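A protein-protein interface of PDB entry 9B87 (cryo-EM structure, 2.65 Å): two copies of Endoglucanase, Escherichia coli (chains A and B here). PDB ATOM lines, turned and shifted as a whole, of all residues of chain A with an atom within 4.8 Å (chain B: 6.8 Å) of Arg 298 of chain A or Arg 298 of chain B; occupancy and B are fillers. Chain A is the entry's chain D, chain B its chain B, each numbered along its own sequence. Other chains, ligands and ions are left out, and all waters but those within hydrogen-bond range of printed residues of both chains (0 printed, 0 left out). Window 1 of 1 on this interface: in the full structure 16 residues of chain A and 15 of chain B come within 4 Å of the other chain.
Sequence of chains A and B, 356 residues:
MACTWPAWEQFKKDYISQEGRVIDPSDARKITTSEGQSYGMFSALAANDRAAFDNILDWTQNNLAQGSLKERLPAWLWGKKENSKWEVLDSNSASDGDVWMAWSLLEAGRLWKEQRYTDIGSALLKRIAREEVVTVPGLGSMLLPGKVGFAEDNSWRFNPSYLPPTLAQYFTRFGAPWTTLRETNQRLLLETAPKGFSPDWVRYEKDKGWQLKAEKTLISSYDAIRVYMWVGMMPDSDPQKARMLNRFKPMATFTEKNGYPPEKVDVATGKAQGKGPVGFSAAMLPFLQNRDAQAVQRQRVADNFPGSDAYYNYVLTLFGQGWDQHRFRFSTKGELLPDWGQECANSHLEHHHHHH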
ATOM      1  N   LEU A 285      25.782  19.927  17.446  1.00  0.00           N
ATOM      2  CA  LEU A 285      26.321  19.137  16.339  1.00  0.00           C
ATOM      3  C   LEU A 285      27.755  18.658  16.559  1.00  0.00           C
ATOM      4  O   LEU A 285      28.027  17.468  16.300  1.00  0.00           O
ATOM      5  CB  LEU A 285      26.184  19.884  15.009  1.00  0.00           C
ATOM      6  CG  LEU A 285      24.725  20.078  14.571  1.00  0.00           C
ATOM      7  CD1 LEU A 285      24.656  21.084  13.447  1.00  0.00           C
ATOM      8  CD2 LEU A 285      24.076  18.703  14.213  1.00  0.00           C
ATOM      9  N   GLN A 294      22.888  13.140  16.101  1.00  0.00           N
ATOM     10  CA  GLN A 294      23.451  14.284  15.345  1.00  0.00           C
ATOM     11  C   GLN A 294      22.502  14.606  14.188  1.00  0.00           C
ATOM     12  O   GLN A 294      22.159  15.794  14.011  1.00  0.00           O
ATOM     13  CB  GLN A 294      24.812  13.939  14.745  1.00  0.00           C
ATOM     14  CG  GLN A 294      26.001  14.217  15.657  1.00  0.00           C
ATOM     15  CD  GLN A 294      27.328  13.942  14.986  1.00  0.00           C
ATOM     16  OE1 GLN A 294      27.389  13.496  13.834  1.00  0.00           O
ATOM     17  NE2 GLN A 294      28.411  14.204  15.703  1.00  0.00           N
ATOM     18  N   ALA A 295      22.098  13.578  13.435  1.00  0.00           N
ATOM     19  CA  ALA A 295      21.247  13.831  12.274  1.00  0.00           C
ATOM     20  C   ALA A 295      19.914  14.463  12.675  1.00  0.00           C
ATOM     21  O   ALA A 295      19.351  15.288  11.936  1.00  0.00           O
ATOM     22  CB  ALA A 295      21.028  12.511  11.518  1.00  0.00           C
ATOM     23  N   VAL A 296      19.382  14.081  13.834  1.00  0.00           N
ATOM     24  CA  VAL A 296      18.144  14.700  14.314  1.00  0.00           C
ATOM     25  C   VAL A 296      18.359  16.194  14.561  1.00  0.00           C
ATOM     26  O   VAL A 296      17.559  17.056  14.132  1.00  0.00           O
ATOM     27  CB  VAL A 296      17.653  13.970  15.580  1.00  0.00           C
ATOM     28  CG1 VAL A 296      16.514  14.709  16.238  1.00  0.00           C
ATOM     29  CG2 VAL A 296      17.197  12.544  15.207  1.00  0.00           C
ATOM     30  N   GLN A 297      19.466  16.530  15.230  1.00  0.00           N
ATOM     31  CA  GLN A 297      19.770  17.941  15.453  1.00  0.00           C
ATOM     32  C   GLN A 297      20.038  18.675  14.137  1.00  0.00           C
ATOM     33  O   GLN A 297      19.633  19.839  13.976  1.00  0.00           O
ATOM     34  CB  GLN A 297      20.958  18.073  16.411  1.00  0.00           C
ATOM     35  CG  GLN A 297      20.650  17.511  17.777  1.00  0.00           C
ATOM     36  CD  GLN A 297      19.309  17.982  18.316  1.00  0.00           C
ATOM     37  OE1 GLN A 297      19.062  19.196  18.460  1.00  0.00           O
ATOM     38  NE2 GLN A 297      18.411  17.034  18.563  1.00  0.00           N
ATOM     39  N   ARG A 298      20.719  18.010  13.193  1.00  0.00           N
ATOM     40  CA  ARG A 298      21.010  18.595  11.884  1.00  0.00           C
ATOM     41  C   ARG A 298      19.720  18.950  11.154  1.00  0.00           C
ATOM     42  O   ARG A 298      19.633  19.996  10.497  1.00  0.00           O
ATOM     43  CB  ARG A 298      21.832  17.606  11.039  1.00  0.00           C
ATOM     44  CG  ARG A 298      22.365  18.110   9.693  1.00  0.00           C
ATOM     45  CD  ARG A 298      23.291  17.043   9.063  1.00  0.00           C
ATOM     46  NE  ARG A 298      24.480  16.794   9.873  1.00  0.00           N
ATOM     47  CZ  ARG A 298      24.767  15.639  10.469  1.00  0.00           C
ATOM     48  NH1 ARG A 298      23.989  14.575  10.332  1.00  0.00           N
ATOM     49  NH2 ARG A 298      25.844  15.563  11.244  1.00  0.00           N
ATOM     50  N   GLN A 299      18.716  18.072  11.259  1.00  0.00           N
ATOM     51  CA  GLN A 299      17.406  18.295  10.583  1.00  0.00           C
ATOM     52  C   GLN A 299      16.673  19.477  11.233  1.00  0.00           C
ATOM     53  O   GLN A 299      16.001  20.226  10.492  1.00  0.00           O
ATOM     54  CB  GLN A 299      16.524  17.048  10.659  1.00  0.00           C
ATOM     55  CG  GLN A 299      15.123  17.239  10.090  1.00  0.00           C
ATOM     56  CD  GLN A 299      14.225  16.036  10.275  1.00  0.00           C
ATOM     57  OE1 GLN A 299      13.207  16.092  10.975  1.00  0.00           O
ATOM     58  NE2 GLN A 299      14.595  14.927   9.653  1.00  0.00           N
ATOM     59  N   ARG A 300      16.791  19.643  12.553  1.00  0.00           N
ATOM     60  CA  ARG A 300      16.183  20.809  13.187  1.00  0.00           C
ATOM     61  C   ARG A 300      16.848  22.111  12.761  1.00  0.00           C
ATOM     62  O   ARG A 300      16.159  23.120  12.547  1.00  0.00           O
ATOM     63  CB  ARG A 300      16.206  20.672  14.702  1.00  0.00           C
ATOM     64  CG  ARG A 300      15.193  21.604  15.337  1.00  0.00           C
ATOM     65  CD  ARG A 300      15.342  21.641  16.831  1.00  0.00           C
ATOM     66  NE  ARG A 300      14.481  22.660  17.416  1.00  0.00           N
ATOM     67  CZ  ARG A 300      14.842  23.417  18.439  1.00  0.00           C
ATOM     68  NH1 ARG A 300      16.012  23.249  19.029  1.00  0.00           N
ATOM     69  NH2 ARG A 300      14.009  24.366  18.875  1.00  0.00           N
ATOM     70  N   VAL A 301      18.185  22.123  12.646  1.00  0.00           N
ATOM     71  CA  VAL A 301      18.850  23.353  12.207  1.00  0.00           C
ATOM     72  C   VAL A 301      18.493  23.659  10.756  1.00  0.00           C
ATOM     73  O   VAL A 301      18.255  24.824  10.387  1.00  0.00           O
ATOM     74  CB  VAL A 301      20.377  23.267  12.396  1.00  0.00           C
ATOM     75  CG1 VAL A 301      21.060  24.546  11.854  1.00  0.00           C
ATOM     76  CG2 VAL A 301      20.704  23.088  13.847  1.00  0.00           C
ATOM     77  N   ALA A 302      18.430  22.618   9.910  1.00  0.00           N
ATOM     78  CA  ALA A 302      18.152  22.864   8.499  1.00  0.00           C
ATOM     79  C   ALA A 302      16.745  23.416   8.291  1.00  0.00           C
ATOM     80  O   ALA A 302      16.532  24.272   7.429  1.00  0.00           O
ATOM     81  CB  ALA A 302      18.336  21.590   7.694  1.00  0.00           C
ATOM     82  N   ASP A 324      29.977  21.366  11.661  1.00  0.00           N
ATOM     83  CA  ASP A 324      29.341  20.188  11.050  1.00  0.00           C
ATOM     84  C   ASP A 324      29.562  20.121   9.541  1.00  0.00           C
ATOM     85  O   ASP A 324      29.500  19.026   8.957  1.00  0.00           O
ATOM     86  CB  ASP A 324      27.842  20.213  11.385  1.00  0.00           C
ATOM     87  CG  ASP A 324      27.114  18.927  11.041  1.00  0.00           C
ATOM     88  OD1 ASP A 324      27.482  17.836  11.546  1.00  0.00           O
ATOM     89  OD2 ASP A 324      26.126  19.026  10.256  1.00  0.00           O
ATOM     90  N   SER B 281      27.879  12.211  -3.787  1.00  0.00           N
ATOM     91  CA  SER B 281      28.224  12.643  -2.440  1.00  0.00           C
ATOM     92  C   SER B 281      27.088  12.368  -1.470  1.00  0.00           C
ATOM     93  O   SER B 281      27.327  11.952  -0.333  1.00  0.00           O
ATOM     94  CB  SER B 281      28.594  14.137  -2.423  1.00  0.00           C
ATOM     95  OG  SER B 281      29.846  14.306  -3.050  1.00  0.00           O
ATOM     96  N   LEU B 285      26.623   9.621   2.184  1.00  0.00           N
ATOM     97  CA  LEU B 285      26.352  10.008   3.570  1.00  0.00           C
ATOM     98  C   LEU B 285      25.977   8.827   4.466  1.00  0.00           C
ATOM     99  O   LEU B 285      26.521   8.731   5.579  1.00  0.00           O
ATOM    100  CB  LEU B 285      25.292  11.107   3.639  1.00  0.00           C
ATOM    101  CG  LEU B 285      25.747  12.449   3.031  1.00  0.00           C
ATOM    102  CD1 LEU B 285      24.545  13.377   2.849  1.00  0.00           C
ATOM    103  CD2 LEU B 285      26.861  13.099   3.847  1.00  0.00           C
ATOM    104  N   ASN B 290      33.146   7.570   9.455  1.00  0.00           N
ATOM    105  CA  ASN B 290      33.834   8.564  10.328  1.00  0.00           C
ATOM    106  C   ASN B 290      32.847   9.703  10.615  1.00  0.00           C
ATOM    107  O   ASN B 290      31.929   9.892   9.789  1.00  0.00           O
ATOM    108  CB  ASN B 290      35.095   9.098   9.661  1.00  0.00           C
ATOM    109  CG  ASN B 290      35.941   9.948  10.578  1.00  0.00           C
ATOM    110  OD1 ASN B 290      35.628  10.091  11.765  1.00  0.00           O
ATOM    111  ND2 ASN B 290      37.021  10.506  10.052  1.00  0.00           N
ATOM    112  N   ARG B 291      33.023  10.448  11.713  1.00  0.00           N
ATOM    113  CA  ARG B 291      32.137  11.618  11.955  1.00  0.00           C
ATOM    114  C   ARG B 291      32.658  12.815  11.145  1.00  0.00           C
ATOM    115  O   ARG B 291      31.866  13.751  10.904  1.00  0.00           O
ATOM    116  CB  ARG B 291      32.115  12.023  13.431  1.00  0.00           C
ATOM    117  CG  ARG B 291      30.861  11.671  14.218  1.00  0.00           C
ATOM    118  CD  ARG B 291      30.717  10.172  14.385  1.00  0.00           C
ATOM    119  NE  ARG B 291      32.019   9.526  14.584  1.00  0.00           N
ATOM    120  CZ  ARG B 291      32.374   8.847  15.664  1.00  0.00           C
ATOM    121  NH1 ARG B 291      31.584   8.824  16.721  1.00  0.00           N
ATOM    122  NH2 ARG B 291      33.522   8.195  15.683  1.00  0.00           N
ATOM    123  N   ALA B 293      34.469  12.513   7.990  1.00  0.00           N
ATOM    124  CA  ALA B 293      34.344  12.276   6.532  1.00  0.00           C
ATOM    125  C   ALA B 293      32.890  12.544   6.190  1.00  0.00           C
ATOM    126  O   ALA B 293      32.630  13.272   5.258  1.00  0.00           O
ATOM    127  CB  ALA B 293      34.694  10.858   6.247  1.00  0.00           C
ATOM    128  N   GLN B 294      31.975  12.035   7.012  1.00  0.00           N
ATOM    129  CA  GLN B 294      30.525  12.208   6.753  1.00  0.00           C
ATOM    130  C   GLN B 294      30.173  13.708   6.664  1.00  0.00           C
ATOM    131  O   GLN B 294      29.024  14.008   6.278  1.00  0.00           O
ATOM    132  CB  GLN B 294      29.783  11.462   7.861  1.00  0.00           C
ATOM    133  CG  GLN B 294      28.339  11.093   7.539  1.00  0.00           C
ATOM    134  CD  GLN B 294      27.644  10.409   8.696  1.00  0.00           C
ATOM    135  OE1 GLN B 294      28.225  10.191   9.765  1.00  0.00           O
ATOM    136  NE2 GLN B 294      26.382  10.060   8.489  1.00  0.00           N
ATOM    137  N   ALA B 295      31.113  14.608   6.992  1.00  0.00           N
ATOM    138  CA  ALA B 295      30.836  16.072   6.964  1.00  0.00           C
ATOM    139  C   ALA B 295      31.592  16.837   5.840  1.00  0.00           C
ATOM    140  O   ALA B 295      31.311  18.036   5.745  1.00  0.00           O
ATOM    141  CB  ALA B 295      30.982  16.611   8.339  1.00  0.00           C
ATOM    142  N   VAL B 296      32.611  16.315   5.146  1.00  0.00           N
ATOM    143  CA  VAL B 296      33.058  16.856   3.861  1.00  0.00           C
ATOM    144  C   VAL B 296      32.008  16.614   2.783  1.00  0.00           C
ATOM    145  O   VAL B 296      31.626  17.528   2.023  1.00  0.00           O
ATOM    146  CB  VAL B 296      34.415  16.254   3.468  1.00  0.00           C
ATOM    147  CG1 VAL B 296      34.757  16.642   2.031  1.00  0.00           C
ATOM    148  CG2 VAL B 296      35.510  16.764   4.414  1.00  0.00           C
ATOM    149  N   GLN B 297      31.528  15.369   2.693  1.00  0.00           N
ATOM    150  CA  GLN B 297      30.473  15.072   1.722  1.00  0.00           C
ATOM    151  C   GLN B 297      29.212  15.875   2.025  1.00  0.00           C
ATOM    152  O   GLN B 297      28.506  16.324   1.108  1.00  0.00           O
ATOM    153  CB  GLN B 297      30.179  13.575   1.736  1.00  0.00           C
ATOM    154  CG  GLN B 297      31.381  12.743   1.294  1.00  0.00           C
ATOM    155  CD  GLN B 297      32.032  13.276   0.030  1.00  0.00           C
ATOM    156  OE1 GLN B 297      31.383  13.377  -1.021  1.00  0.00           O
ATOM    157  NE2 GLN B 297      33.306  13.674   0.134  1.00  0.00           N
ATOM    158  N   ARG B 298      28.909  16.049   3.314  1.00  0.00           N
ATOM    159  CA  ARG B 298      27.735  16.810   3.712  1.00  0.00           C
ATOM    160  C   ARG B 298      27.845  18.243   3.202  1.00  0.00           C
ATOM    161  O   ARG B 298      26.870  18.822   2.707  1.00  0.00           O
ATOM    162  CB  ARG B 298      27.600  16.803   5.244  1.00  0.00           C
ATOM    163  CG  ARG B 298      26.305  17.449   5.771  1.00  0.00           C
ATOM    164  CD  ARG B 298      26.169  17.238   7.277  1.00  0.00           C
ATOM    165  NE  ARG B 298      26.037  15.811   7.599  1.00  0.00           N
ATOM    166  CZ  ARG B 298      26.921  15.117   8.306  1.00  0.00           C
ATOM    167  NH1 ARG B 298      27.997  15.696   8.835  1.00  0.00           N
ATOM    168  NH2 ARG B 298      26.747  13.800   8.454  1.00  0.00           N
ATOM    169  N   GLN B 299      29.041  18.811   3.294  1.00  0.00           N
ATOM    170  CA  GLN B 299      29.255  20.163   2.799  1.00  0.00           C
ATOM    171  C   GLN B 299      29.041  20.212   1.292  1.00  0.00           C
ATOM    172  O   GLN B 299      28.434  21.151   0.762  1.00  0.00           O
ATOM    173  CB  GLN B 299      30.670  20.621   3.150  1.00  0.00           C
ATOM    174  CG  GLN B 299      30.936  22.059   2.718  1.00  0.00           C
ATOM    175  CD  GLN B 299      32.387  22.449   2.826  1.00  0.00           C
ATOM    176  OE1 GLN B 299      33.036  22.812   1.833  1.00  0.00           O
ATOM    177  NE2 GLN B 299      32.918  22.371   4.038  1.00  0.00           N
ATOM    178  N   ARG B 300      29.541  19.201   0.581  1.00  0.00           N
ATOM    179  CA  ARG B 300      29.413  19.224  -0.871  1.00  0.00           C
ATOM    180  C   ARG B 300      27.949  19.155  -1.306  1.00  0.00           C
ATOM    181  O   ARG B 300      27.550  19.846  -2.252  1.00  0.00           O
ATOM    182  CB  ARG B 300      30.224  18.089  -1.489  1.00  0.00           C
ATOM    183  CG  ARG B 300      30.518  18.359  -2.939  1.00  0.00           C
ATOM    184  CD  ARG B 300      31.113  17.182  -3.614  1.00  0.00           C
ATOM    185  NE  ARG B 300      31.211  17.454  -5.038  1.00  0.00           N
ATOM    186  CZ  ARG B 300      30.958  16.544  -5.963  1.00  0.00           C
ATOM    187  NH1 ARG B 300      30.507  15.349  -5.631  1.00  0.00           N
ATOM    188  NH2 ARG B 300      31.107  16.860  -7.248  1.00  0.00           N
ATOM    189  N   VAL B 301      27.135  18.335  -0.625  1.00  0.00           N
ATOM    190  CA  VAL B 301      25.707  18.274  -0.935  1.00  0.00           C
ATOM    191  C   VAL B 301      25.031  19.606  -0.624  1.00  0.00           C
ATOM    192  O   VAL B 301      24.241  20.131  -1.427  1.00  0.00           O
ATOM    193  CB  VAL B 301      25.037  17.119  -0.170  1.00  0.00           C
ATOM    194  CG1 VAL B 301      23.549  17.105  -0.428  1.00  0.00           C
ATOM    195  CG2 VAL B 301      25.655  15.791  -0.605  1.00  0.00           C
ATOM    196  N   ALA B 302      25.328  20.170   0.550  1.00  0.00           N
ATOM    197  CA  ALA B 302      24.708  21.439   0.938  1.00  0.00           C
ATOM    198  C   ALA B 302      25.027  22.548  -0.056  1.00  0.00           C
ATOM    199  O   ALA B 302      24.138  23.322  -0.430  1.00  0.00           O
ATOM    200  CB  ALA B 302      25.169  21.845   2.346  1.00  0.00           C
ATOM    201  N   ASP B 303      26.274  22.630  -0.517  1.00  0.00           N
ATOM    202  CA  ASP B 303      26.678  23.756  -1.355  1.00  0.00           C
ATOM    203  C   ASP B 303      26.402  23.572  -2.844  1.00  0.00           C
ATOM    204  O   ASP B 303      26.501  24.551  -3.595  1.00  0.00           O
ATOM    205  CB  ASP B 303      28.158  24.053  -1.165  1.00  0.00           C
ATOM    206  CG  ASP B 303      28.454  24.639   0.193  1.00  0.00           C
ATOM    207  OD1 ASP B 303      27.500  24.883   0.976  1.00  0.00           O
ATOM    208  OD2 ASP B 303      29.646  24.845   0.474  1.00  0.00           O
ATOM    209  N   GLN B 321      20.835  12.333   1.516  1.00  0.00           N
ATOM    210  CA  GLN B 321      20.668  13.398   2.491  1.00  0.00           C
ATOM    211  C   GLN B 321      19.435  13.175   3.360  1.00  0.00           C
ATOM    212  O   GLN B 321      19.462  13.524   4.542  1.00  0.00           O
ATOM    213  CB  GLN B 321      20.598  14.761   1.801  1.00  0.00           C
ATOM    214  CG  GLN B 321      20.417  15.893   2.798  1.00  0.00           C
ATOM    215  CD  GLN B 321      20.204  17.241   2.141  1.00  0.00           C
ATOM    216  OE1 GLN B 321      19.130  17.491   1.595  1.00  0.00           O
ATOM    217  NE2 GLN B 321      21.172  18.146   2.280  1.00  0.00           N
ATOM    218  N   TRP B 323      18.359  10.313   4.508  1.00  0.00           N
ATOM    219  CA  TRP B 323      18.822   9.433   5.614  1.00  0.00           C
ATOM    220  C   TRP B 323      19.730  10.227   6.558  1.00  0.00           C
ATOM    221  O   TRP B 323      19.557  10.129   7.797  1.00  0.00           O
ATOM    222  CB  TRP B 323      19.541   8.189   5.084  1.00  0.00           C
ATOM    223  CG  TRP B 323      19.590   7.058   6.077  1.00  0.00           C
ATOM    224  CD1 TRP B 323      18.664   6.070   6.238  1.00  0.00           C
ATOM    225  CD2 TRP B 323      20.619   6.806   7.057  1.00  0.00           C
ATOM    226  NE1 TRP B 323      19.046   5.216   7.238  1.00  0.00           N
ATOM    227  CE2 TRP B 323      20.238   5.643   7.761  1.00  0.00           C
ATOM    228  CE3 TRP B 323      21.813   7.444   7.407  1.00  0.00           C
ATOM    229  CZ2 TRP B 323      21.012   5.111   8.790  1.00  0.00           C
ATOM    230  CZ3 TRP B 323      22.574   6.918   8.426  1.00  0.00           C
ATOM    231  CH2 TRP B 323      22.177   5.768   9.107  1.00  0.00           C
ATOM    232  N   ASP B 324      20.654  11.010   6.005  1.00  0.00           N
ATOM    233  CA  ASP B 324      21.519  11.844   6.837  1.00  0.00           C
ATOM    234  C   ASP B 324      20.717  12.764   7.756  1.00  0.00           C
ATOM    235  O   ASP B 324      21.216  13.169   8.814  1.00  0.00           O
ATOM    236  CB  ASP B 324      22.436  12.664   5.930  1.00  0.00           C
ATOM    237  CG  ASP B 324      23.549  13.339   6.690  1.00  0.00           C
ATOM    238  OD1 ASP B 324      24.303  12.598   7.348  1.00  0.00           O
ATOM    239  OD2 ASP B 324      23.697  14.586   6.585  1.00  0.00           O
ATOM    240  N   GLN B 325      19.461  13.065   7.427  1.00  0.00           N
ATOM    241  CA  GLN B 325      18.680  14.004   8.282  1.00  0.00           C
ATOM    242  C   GLN B 325      17.606  13.225   9.059  1.00  0.00           C
ATOM    243  O   GLN B 325      16.736  13.888   9.664  1.00  0.00           O
ATOM    244  CB  GLN B 325      18.026  15.155   7.516  1.00  0.00           C
ATOM    245  CG  GLN B 325      19.002  16.228   7.051  1.00  0.00           C
ATOM    246  CD  GLN B 325      18.327  17.354   6.300  1.00  0.00           C
ATOM    247  OE1 GLN B 325      17.116  17.333   6.057  1.00  0.00           O
ATOM    248  NE2 GLN B 325      19.113  18.348   5.915  1.00  0.00           N
ATOM    249  N   ARG B 327      15.181  11.286   7.896  1.00  0.00           N
ATOM    250  CA  ARG B 327      13.864  11.333   7.275  1.00  0.00           C
ATOM    251  C   ARG B 327      13.187   9.968   7.244  1.00  0.00           C
ATOM    252  O   ARG B 327      11.982   9.891   6.942  1.00  0.00           O
ATOM    253  CB  ARG B 327      13.976  11.852   5.847  1.00  0.00           C
ATOM    254  CG  ARG B 327      14.557  13.261   5.729  1.00  0.00           C
ATOM    255  CD  ARG B 327      13.638  14.323   6.224  1.00  0.00           C
ATOM    256  NE  ARG B 327      14.337  15.608   6.155  1.00  0.00           N
ATOM    257  CZ  ARG B 327      13.867  16.741   6.657  1.00  0.00           C
ATOM    258  NH1 ARG B 327      12.658  16.803   7.200  1.00  0.00           N
ATOM    259  NH2 ARG B 327      14.621  17.837   6.590  1.00  0.00           N
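OD2 of Asp 324 of chain B lies within salt-bridge range of NE of Arg 298 of chain B, at 2.8 Å. NE of Arg 298 of chain A lies within salt-bridge range of OD2 of Asp 324 of chain A, 2.8 Å away. The side-chain amide nitrogen (NE2) of Gln 294 of chain B sits at hydrogen-bond distance from the side-chain carboxylate (OD1) of Asp 324 of chain B (3.5 Å). NE2 of Gln 294 of chain A sits at hydrogen-bond distance from O of Leu 285 of chain A (3.3 Å). The backbone carbonyl oxygen (O) of Gln 294 of chain B lies close to the guanidinium group (NH2) of Arg 298 of chain B (3.2 Å). The side-chain amide oxygen of Gln 325 of chain B sits at hydrogen-bond distance from the guanidinium group of Arg 327 of chain B.
Hydrophobic or aromatic side chains of chain B that line the printed part of chain A: Ala 295. Printed residues of chain A that touch a printed residue of chain B: Gln 294, Ala 295, Arg 298, Gln 299, Ala 302 and Asp 324. Among the printed residues, 10 pairs touch across the chains. Among the printed residues, Asp or Glu carboxylates within 4 Å of a Lys or Arg side-chain nitrogen of the other chain: Arg 298 of chain A with Asp 324 of chain B (3.6 Å) and Asp 324 of chain A with Arg 298 of chain B (3.5 Å).
NE2 of Gln 294 of chain A touches CG of Arg 291 of chain B, at 3.8 Å. CB of Ala 295 of chain A touches O of Asp 324 of chain B (2.8 Å). O of Ala 295 of chain A touches O of Gln 325 of chain B, 3.7 Å away. Arg 327 of chain B touches Gln 299 of chain A. NE2 of Gln 325 of chain B touches CB of Ala 302 of chain A, 3.8 Å away. Asp 324 of chain A touches Ala 295 of chain B (O to CB, 2.9 Å).
Ala 295 of chain A touches Asp 324 of chain B, and with the chains exchanged Asp 324 of chain A touches Ala 295 of chain B. Arg 298 of chain B touches its own counterpart, Arg 298 of chain A. Arg 298 of chain A touches Asp 324 of chain B, and with the chains exchanged Asp 324 of chain A touches Arg 298 of chain B. Of the 10 pairs that touch across the chains among the printed residues, 5 have their exchanged pair printed and touching as well.
Arg 298 of chain A touches just these residues of chain B: Arg 298 (2.9 Å) and Asp 324 (3.5 Å). Arg 298 of chain B touches just these residues of chain A: Arg 298 and Asp 324. Printed residues of chain B within 4 Å of Ala 295 of chain A: Asp 324 (2.8 Å) and Gln 325 (3.7 Å). Printed residues of chain B within 4 Å of Gln 299 of chain A: Gln 325 and Arg 327. Leu 285 of chain A touches none of the printed residues of chain B. Gln 294 of chain B touches none of the printed residues of chain A. The nearest printed residue of chain A that does not touch Arg 298 of chain B is Gln 294 of chain A (5.4 Å).
The guanidinium group of Arg 298 of chain A lies within salt-bridge range of the side-chain carboxylate of Asp 324 of chain B. The side-chain carboxylate (OD1) of Asp 324 of chain A is in salt-bridge range of the guanidinium group (NH1) of Arg 298 of chain B (3.5 Å). The side-chain amide nitrogen (NE2) of Gln 299 of chain A lies close to the backbone carbonyl oxygen (O) of Gln 325 of chain B (2.4 Å). NE of Arg 298 of chain B sits close to NE of Arg 298 of chain A (2.9 Å).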
